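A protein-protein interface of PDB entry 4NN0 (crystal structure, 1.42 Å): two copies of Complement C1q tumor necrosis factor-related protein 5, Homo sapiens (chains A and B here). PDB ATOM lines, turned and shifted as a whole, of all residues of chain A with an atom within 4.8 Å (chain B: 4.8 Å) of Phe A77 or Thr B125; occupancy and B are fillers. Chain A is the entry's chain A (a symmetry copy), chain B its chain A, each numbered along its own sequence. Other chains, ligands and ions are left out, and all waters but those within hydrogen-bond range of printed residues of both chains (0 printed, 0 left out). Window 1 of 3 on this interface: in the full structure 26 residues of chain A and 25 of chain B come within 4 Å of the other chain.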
ATOM      1  N   LEU A  63     -35.206  31.054  16.877  1.00  0.00           N
ATOM      2  CA  LEU A  63     -34.630  31.148  15.567  1.00  0.00           C
ATOM      3  C   LEU A  63     -33.565  30.090  15.397  1.00  0.00           C
ATOM      4  O   LEU A  63     -32.655  29.996  16.210  1.00  0.00           O
ATOM      5  CB  LEU A  63     -34.023  32.537  15.276  1.00  0.00           C
ATOM      6  CG  LEU A  63     -33.344  32.706  13.957  1.00  0.00           C
ATOM      7  CD1 LEU A  63     -34.261  32.448  12.755  1.00  0.00           C
ATOM      8  CD2 LEU A  63     -32.739  34.124  13.882  1.00  0.00           C
ATOM      9  N   GLN A  64     -33.696  29.293  14.336  1.00  0.00           N
ATOM     10  CA  GLN A  64     -32.687  28.380  13.881  1.00  0.00           C
ATOM     11  C   GLN A  64     -32.349  28.759  12.455  1.00  0.00           C
ATOM     12  O   GLN A  64     -33.260  28.891  11.620  1.00  0.00           O
ATOM     13  CB  GLN A  64     -33.157  26.922  13.983  1.00  0.00           C
ATOM     14  CG  GLN A  64     -32.009  25.888  13.879  1.00  0.00           C
ATOM     15  CD  GLN A  64     -31.481  25.713  12.455  1.00  0.00           C
ATOM     16  OE1 GLN A  64     -32.222  25.898  11.445  1.00  0.00           O
ATOM     17  NE2 GLN A  64     -30.249  25.410  12.323  1.00  0.00           N
ATOM     18  N   PHE A  65     -31.096  29.014  12.129  1.00  0.00           N
ATOM     19  CA  PHE A  65     -30.716  29.183  10.757  1.00  0.00           C
ATOM     20  C   PHE A  65     -29.440  28.459  10.412  1.00  0.00           C
ATOM     21  O   PHE A  65     -28.547  28.272  11.265  1.00  0.00           O
ATOM     22  CB  PHE A  65     -30.623  30.675  10.324  1.00  0.00           C
ATOM     23  CG  PHE A  65     -29.515  31.473  10.976  1.00  0.00           C
ATOM     24  CD1 PHE A  65     -28.205  31.409  10.493  1.00  0.00           C
ATOM     25  CD2 PHE A  65     -29.768  32.280  12.065  1.00  0.00           C
ATOM     26  CE1 PHE A  65     -27.176  32.111  11.064  1.00  0.00           C
ATOM     27  CE2 PHE A  65     -28.752  33.014  12.626  1.00  0.00           C
ATOM     28  CZ  PHE A  65     -27.446  32.911  12.140  1.00  0.00           C
ATOM     29  N   LEU A  67     -26.267  28.700   7.607  1.00  0.00           N
ATOM     30  CA  LEU A  67     -25.510  29.283   6.505  1.00  0.00           C
ATOM     31  C   LEU A  67     -25.266  28.138   5.549  1.00  0.00           C
ATOM     32  O   LEU A  67     -24.727  27.113   5.948  1.00  0.00           O
ATOM     33  CB  LEU A  67     -24.166  29.794   6.978  1.00  0.00           C
ATOM     34  CG  LEU A  67     -24.085  31.239   7.394  1.00  0.00           C
ATOM     35  CD1 LEU A  67     -22.796  31.508   8.125  1.00  0.00           C
ATOM     36  CD2 LEU A  67     -24.096  32.055   6.146  1.00  0.00           C
ATOM     37  N   ALA A  75     -22.751  25.754   8.522  1.00  0.00           N
ATOM     38  CA  ALA A  75     -22.830  25.887   9.971  1.00  0.00           C
ATOM     39  C   ALA A  75     -24.251  26.283  10.338  1.00  0.00           C
ATOM     40  O   ALA A  75     -24.911  26.999   9.574  1.00  0.00           O
ATOM     41  CB  ALA A  75     -21.819  26.903  10.495  1.00  0.00           C
ATOM     42  N   SER A  76     -24.690  25.830  11.493  1.00  0.00           N
ATOM     43  CA  SER A  76     -26.060  26.001  11.974  1.00  0.00           C
ATOM     44  C   SER A  76     -26.065  26.706  13.317  1.00  0.00           C
ATOM     45  O   SER A  76     -25.207  26.394  14.154  1.00  0.00           O
ATOM     46  CB  SER A  76     -26.676  24.599  12.114  1.00  0.00           C
ATOM     47  OG  SER A  76     -26.705  23.896  10.871  1.00  0.00           O
ATOM     48  N   PHE A  77     -27.068  27.554  13.560  1.00  0.00           N
ATOM     49  CA  PHE A  77     -27.129  28.332  14.764  1.00  0.00           C
ATOM     50  C   PHE A  77     -28.542  28.372  15.319  1.00  0.00           C
ATOM     51  O   PHE A  77     -29.523  28.209  14.568  1.00  0.00           O
ATOM     52  CB  PHE A  77     -26.615  29.748  14.477  1.00  0.00           C
ATOM     53  CG  PHE A  77     -25.182  29.740  13.984  1.00  0.00           C
ATOM     54  CD1 PHE A  77     -24.129  29.602  14.887  1.00  0.00           C
ATOM     55  CD2 PHE A  77     -24.894  29.751  12.654  1.00  0.00           C
ATOM     56  CE1 PHE A  77     -22.820  29.497  14.441  1.00  0.00           C
ATOM     57  CE2 PHE A  77     -23.608  29.648  12.193  1.00  0.00           C
ATOM     58  CZ  PHE A  77     -22.555  29.545  13.088  1.00  0.00           C
ATOM     59  N   PHE A  78     -28.676  28.614  16.609  1.00  0.00           N
ATOM     60  CA  PHE A  78     -29.942  28.590  17.296  1.00  0.00           C
ATOM     61  C   PHE A  78     -29.967  29.490  18.499  1.00  0.00           C
ATOM     62  O   PHE A  78     -28.978  29.570  19.262  1.00  0.00           O
ATOM     63  CB  PHE A  78     -30.273  27.155  17.745  1.00  0.00           C
ATOM     64  CG  PHE A  78     -31.591  27.042  18.519  1.00  0.00           C
ATOM     65  CD1 PHE A  78     -32.804  26.886  17.823  1.00  0.00           C
ATOM     66  CD2 PHE A  78     -31.663  27.119  19.899  1.00  0.00           C
ATOM     67  CE1 PHE A  78     -34.003  26.819  18.507  1.00  0.00           C
ATOM     68  CE2 PHE A  78     -32.838  27.050  20.573  1.00  0.00           C
ATOM     69  CZ  PHE A  78     -34.024  26.876  19.882  1.00  0.00           C
ATOM     70  N   GLN A  79     -31.097  30.169  18.721  1.00  0.00           N
ATOM     71  CA  GLN A  79     -31.349  30.882  19.937  1.00  0.00           C
ATOM     72  C   GLN A  79     -32.768  30.639  20.417  1.00  0.00           C
ATOM     73  O   GLN A  79     -33.758  30.943  19.698  1.00  0.00           O
ATOM     74  CB  GLN A  79     -31.155  32.392  19.749  1.00  0.00           C
ATOM     75  CG  GLN A  79     -31.571  33.243  20.935  1.00  0.00           C
ATOM     76  CD  GLN A  79     -30.745  32.975  22.218  1.00  0.00           C
ATOM     77  OE1 GLN A  79     -29.524  32.971  22.193  1.00  0.00           O
ATOM     78  NE2 GLN A  79     -31.435  32.768  23.302  1.00  0.00           N
ATOM     79  N   LEU A  90     -29.062  36.616  17.999  1.00  0.00           N
ATOM     80  CA  LEU A  90     -28.353  35.445  17.560  1.00  0.00           C
ATOM     81  C   LEU A  90     -27.388  35.804  16.454  1.00  0.00           C
ATOM     82  O   LEU A  90     -27.818  36.324  15.425  1.00  0.00           O
ATOM     83  CB  LEU A  90     -29.316  34.372  17.022  1.00  0.00           C
ATOM     84  CG  LEU A  90     -28.661  33.125  16.419  1.00  0.00           C
ATOM     85  CD1 LEU A  90     -27.777  32.359  17.415  1.00  0.00           C
ATOM     86  CD2 LEU A  90     -29.729  32.204  15.851  1.00  0.00           C
ATOM     87  N   SER A  91     -26.105  35.530  16.617  1.00  0.00           N
ATOM     88  CA  SER A  91     -25.135  35.682  15.549  1.00  0.00           C
ATOM     89  C   SER A  91     -24.528  34.364  15.146  1.00  0.00           C
ATOM     90  O   SER A  91     -24.364  33.451  15.960  1.00  0.00           O
ATOM     91  CB  SER A  91     -24.032  36.706  15.886  1.00  0.00           C
ATOM     92  OG  SER A  91     -24.584  37.995  16.125  1.00  0.00           O
ATOM     93  N   GLY A  92     -24.127  34.264  13.890  1.00  0.00           N
ATOM     94  CA  GLY A  92     -23.425  33.100  13.398  1.00  0.00           C
ATOM     95  C   GLY A  92     -22.482  33.496  12.321  1.00  0.00           C
ATOM     96  O   GLY A  92     -22.669  34.521  11.663  1.00  0.00           O
ATOM     97  N   GLY A  93     -21.438  32.735  12.079  1.00  0.00           N
ATOM     98  CA  GLY A  93     -20.474  33.046  11.083  1.00  0.00           C
ATOM     99  C   GLY A  93     -19.558  31.857  10.841  1.00  0.00           C
ATOM    100  O   GLY A  93     -19.450  30.950  11.702  1.00  0.00           O
ATOM    101  N   ALA A  94     -18.871  31.894   9.718  1.00  0.00           N
ATOM    102  CA  ALA A  94     -17.966  30.801   9.312  1.00  0.00           C
ATOM    103  C   ALA A  94     -17.187  31.271   8.090  1.00  0.00           C
ATOM    104  O   ALA A  94     -17.586  32.260   7.454  1.00  0.00           O
ATOM    105  CB  ALA A  94     -18.687  29.497   9.039  1.00  0.00           C
ATOM    106  N   ALA B   7     -13.419  26.340  11.746  1.00  0.00           N
ATOM    107  CA  ALA B   7     -13.693  24.993  12.249  1.00  0.00           C
ATOM    108  C   ALA B   7     -14.867  24.986  13.193  1.00  0.00           C
ATOM    109  O   ALA B   7     -15.217  26.033  13.784  1.00  0.00           O
ATOM    110  CB  ALA B   7     -12.458  24.407  12.900  1.00  0.00           C
ATOM    111  N   LYS B   8     -15.465  23.824  13.373  1.00  0.00           N
ATOM    112  CA  LYS B   8     -16.628  23.641  14.201  1.00  0.00           C
ATOM    113  C   LYS B   8     -16.399  22.563  15.249  1.00  0.00           C
ATOM    114  O   LYS B   8     -15.585  21.669  15.067  1.00  0.00           O
ATOM    115  CB  LYS B   8     -17.876  23.219  13.363  1.00  0.00           C
ATOM    116  CG  LYS B   8     -18.234  24.035  12.146  1.00  0.00           C
ATOM    117  CD  LYS B   8     -19.478  23.440  11.469  1.00  0.00           C
ATOM    118  CE  LYS B   8     -19.224  22.156  10.682  1.00  0.00           C
ATOM    119  NZ  LYS B   8     -20.221  21.992   9.589  1.00  0.00           N
ATOM    120  N   PHE B  24     -12.146  22.428  18.267  1.00  0.00           N
ATOM    121  CA  PHE B  24     -13.001  22.629  17.089  1.00  0.00           C
ATOM    122  C   PHE B  24     -12.389  21.758  15.994  1.00  0.00           C
ATOM    123  O   PHE B  24     -11.454  22.152  15.282  1.00  0.00           O
ATOM    124  CB  PHE B  24     -13.071  24.098  16.657  1.00  0.00           C
ATOM    125  CG  PHE B  24     -13.626  25.045  17.703  1.00  0.00           C
ATOM    126  CD1 PHE B  24     -12.797  25.526  18.685  1.00  0.00           C
ATOM    127  CD2 PHE B  24     -14.966  25.418  17.735  1.00  0.00           C
ATOM    128  CE1 PHE B  24     -13.238  26.411  19.649  1.00  0.00           C
ATOM    129  CE2 PHE B  24     -15.440  26.280  18.683  1.00  0.00           C
ATOM    130  CZ  PHE B  24     -14.581  26.776  19.681  1.00  0.00           C
ATOM    131  N   ALA B  53     -13.104  35.272  15.364  1.00  0.00           N
ATOM    132  CA  ALA B  53     -14.485  35.236  15.806  1.00  0.00           C
ATOM    133  C   ALA B  53     -14.911  33.872  16.263  1.00  0.00           C
ATOM    134  O   ALA B  53     -14.573  32.870  15.591  1.00  0.00           O
ATOM    135  CB  ALA B  53     -15.419  35.707  14.714  1.00  0.00           C
ATOM    136  N   VAL B  54     -15.636  33.823  17.365  1.00  0.00           N
ATOM    137  CA  VAL B  54     -16.251  32.620  17.870  1.00  0.00           C
ATOM    138  C   VAL B  54     -17.757  32.826  17.872  1.00  0.00           C
ATOM    139  O   VAL B  54     -18.230  33.852  18.371  1.00  0.00           O
ATOM    140  CB  VAL B  54     -15.768  32.306  19.294  1.00  0.00           C
ATOM    141  CG1 VAL B  54     -16.528  31.109  19.890  1.00  0.00           C
ATOM    142  CG2 VAL B  54     -14.269  32.099  19.293  1.00  0.00           C
ATOM    143  N   HIS B  55     -18.516  31.871  17.318  1.00  0.00           N
ATOM    144  CA  HIS B  55     -19.970  31.913  17.329  1.00  0.00           C
ATOM    145  C   HIS B  55     -20.440  30.640  17.977  1.00  0.00           C
ATOM    146  O   HIS B  55     -20.346  29.573  17.326  1.00  0.00           O
ATOM    147  CB  HIS B  55     -20.545  32.078  15.910  1.00  0.00           C
ATOM    148  CG  HIS B  55     -20.095  33.319  15.230  1.00  0.00           C
ATOM    149  ND1 HIS B  55     -20.630  34.562  15.501  1.00  0.00           N
ATOM    150  CD2 HIS B  55     -19.135  33.511  14.297  1.00  0.00           C
ATOM    151  CE1 HIS B  55     -20.037  35.457  14.730  1.00  0.00           C
ATOM    152  NE2 HIS B  55     -19.121  34.853  13.995  1.00  0.00           N
ATOM    153  N   LYS B 121     -28.544  20.299  14.721  1.00  0.00           N
ATOM    154  CA  LYS B 121     -28.882  21.598  14.092  1.00  0.00           C
ATOM    155  C   LYS B 121     -28.300  22.807  14.833  1.00  0.00           C
ATOM    156  O   LYS B 121     -28.806  23.917  14.676  1.00  0.00           O
ATOM    157  CB  LYS B 121     -30.395  21.755  13.908  1.00  0.00           C
ATOM    158  CG  LYS B 121     -31.029  20.759  12.933  1.00  0.00           C
ATOM    159  CD  LYS B 121     -30.454  20.778  11.556  1.00  0.00           C
ATOM    160  CE  LYS B 121     -30.523  22.077  10.816  1.00  0.00           C
ATOM    161  NZ  LYS B 121     -30.149  21.901   9.337  1.00  0.00           N
ATOM    162  N   THR B 122     -27.246  22.605  15.635  1.00  0.00           N
ATOM    163  CA  THR B 122     -26.561  23.723  16.250  1.00  0.00           C
ATOM    164  C   THR B 122     -25.074  23.499  16.192  1.00  0.00           C
ATOM    165  O   THR B 122     -24.589  22.329  16.299  1.00  0.00           O
ATOM    166  CB  THR B 122     -26.960  23.981  17.722  1.00  0.00           C
ATOM    167  OG1 THR B 122     -26.331  23.052  18.625  1.00  0.00           O
ATOM    168  CG2 THR B 122     -28.445  24.012  17.952  1.00  0.00           C
ATOM    169  N   ASP B 123     -24.322  24.573  16.062  1.00  0.00           N
ATOM    170  CA  ASP B 123     -22.872  24.505  15.986  1.00  0.00           C
ATOM    171  C   ASP B 123     -22.223  25.551  16.886  1.00  0.00           C
ATOM    172  O   ASP B 123     -22.837  26.550  17.267  1.00  0.00           O
ATOM    173  CB  ASP B 123     -22.400  24.746  14.548  1.00  0.00           C
ATOM    174  CG  ASP B 123     -22.595  23.546  13.651  1.00  0.00           C
ATOM    175  OD1 ASP B 123     -22.099  22.444  13.990  1.00  0.00           O
ATOM    176  OD2 ASP B 123     -23.179  23.725  12.555  1.00  0.00           O
ATOM    177  N   SER B 124     -20.936  25.356  17.124  1.00  0.00           N
ATOM    178  CA  SER B 124     -20.046  26.385  17.670  1.00  0.00           C
ATOM    179  C   SER B 124     -18.842  26.458  16.754  1.00  0.00           C
ATOM    180  O   SER B 124     -18.186  25.445  16.498  1.00  0.00           O
ATOM    181  CB  SER B 124     -19.631  26.069  19.094  1.00  0.00           C
ATOM    182  OG  SER B 124     -20.756  26.069  19.976  1.00  0.00           O
ATOM    183  N   THR B 125     -18.564  27.628  16.187  1.00  0.00           N
ATOM    184  CA  THR B 125     -17.501  27.831  15.243  1.00  0.00           C
ATOM    185  C   THR B 125     -16.407  28.740  15.763  1.00  0.00           C
ATOM    186  O   THR B 125     -16.671  29.662  16.574  1.00  0.00           O
ATOM    187  CB  THR B 125     -18.003  28.422  13.899  1.00  0.00           C
ATOM    188  OG1 THR B 125     -18.455  29.774  14.087  1.00  0.00           O
ATOM    189  CG2 THR B 125     -19.137  27.597  13.299  1.00  0.00           C
ATOM    190  N   PHE B 126     -15.187  28.516  15.290  1.00  0.00           N
ATOM    191  CA  PHE B 126     -14.012  29.342  15.557  1.00  0.00           C
ATOM    192  C   PHE B 126     -13.366  29.621  14.223  1.00  0.00           C
ATOM    193  O   PHE B 126     -13.097  28.699  13.453  1.00  0.00           O
ATOM    194  CB  PHE B 126     -13.062  28.576  16.489  1.00  0.00           C
ATOM    195  CG  PHE B 126     -11.727  29.213  16.808  1.00  0.00           C
ATOM    196  CD1 PHE B 126     -11.577  30.576  16.959  1.00  0.00           C
ATOM    197  CD2 PHE B 126     -10.628  28.411  17.057  1.00  0.00           C
ATOM    198  CE1 PHE B 126     -10.353  31.126  17.302  1.00  0.00           C
ATOM    199  CE2 PHE B 126      -9.432  28.950  17.370  1.00  0.00           C
ATOM    200  CZ  PHE B 126      -9.287  30.306  17.522  1.00  0.00           C
ATOM    201  N   SER B 127     -13.168  30.889  13.910  1.00  0.00           N
ATOM    202  CA  SER B 127     -12.635  31.329  12.657  1.00  0.00           C
ATOM    203  C   SER B 127     -11.591  32.430  12.873  1.00  0.00           C
ATOM    204  O   SER B 127     -11.693  33.190  13.854  1.00  0.00           O
ATOM    205  CB  SER B 127     -13.742  31.902  11.740  1.00  0.00           C
ATOM    206  OG  SER B 127     -14.845  31.065  11.596  1.00  0.00           O
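Phe A77 touches just these residues of chain B: His B55 and Thr B125.
Printed residues of chain B within 4 Å of Ser A91: His B55.
Of the printed residues of chain A, His B55 touches Phe A77, Ser A91, Gly A92 and Gly A93.
Printed residues of chain A within 4 Å of Lys B121: Gln A64 and Ser A76.
Of the printed residues of chain A, Thr B122 touches Ser A76 (3.5 Å) and Phe A78 (3.6 Å).
Of the printed residues of chain A, Ser B127 touches Ala A94 (3.9 Å).
The nearest residue of chain A that does not touch Thr B125 is Ala A94 (4.7 Å).
The nearest printed residue of chain B that does not touch Phe A78 is Lys B121 (4.7 Å).
Printed residues of chain B that touch a printed residue of chain A: His B55, Lys B121, Thr B122, Asp B123, Thr B125 and Ser B127.
Hydrophobic or aromatic side chains of chain A that line the printed part of chain B: Ala A75, Phe A77 and Phe A78.
CA of Ala A75 touches OD2 of Asp B123, at 3.4 Å.
Ala A75 touches Thr B125.
Lys B121 touches Ser A76.
O of Ser A76 touches C of Thr B122, 3.5 Å away.
Phe A77 touches His B55 (CE1 to CB, 3.7 Å).
Phe A78 touches Thr B122 (CB to CG2, 3.6 Å).
His B55 touches Ser A91.
Gly A92 touches His B55 (C to CG, 3.8 Å).
His B55 touches Gly A93 (CD2 to N, 3.3 Å).
Ser B127 touches Ala A94 (OG to CA, 3.9 Å).
N of Ala B53 is in hydrogen-bond range of O of Ser B127, at 2.9 Å.
O of Ala A75 sits at hydrogen-bond distance from N of Leu A67, 2.9 Å away.
The backbone NH of Phe A77 sits at hydrogen-bond distance from the backbone carbonyl oxygen of Phe A65, 2.8 Å away.
The backbone carbonyl oxygen (O) of His B55 sits at hydrogen-bond distance from the backbone NH (N) of Thr B125 (2.9 Å).
The backbone carbonyl oxygen (O) of Lys B121 is in hydrogen-bond range of the side-chain amide nitrogen (NE2) of Gln A64.
The backbone NH of Asp B123 sits at hydrogen-bond distance from the backbone carbonyl oxygen of Ser A76 (2.8 Å).
The backbone carbonyl oxygen of Gly A93 is in hydrogen-bond range of the side-chain hydroxyl of Thr B125.
No position is printed for both chains.
Of the 14 pairs that touch across the chains among the printed residues, none has its exchanged pair printed and touching as well.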
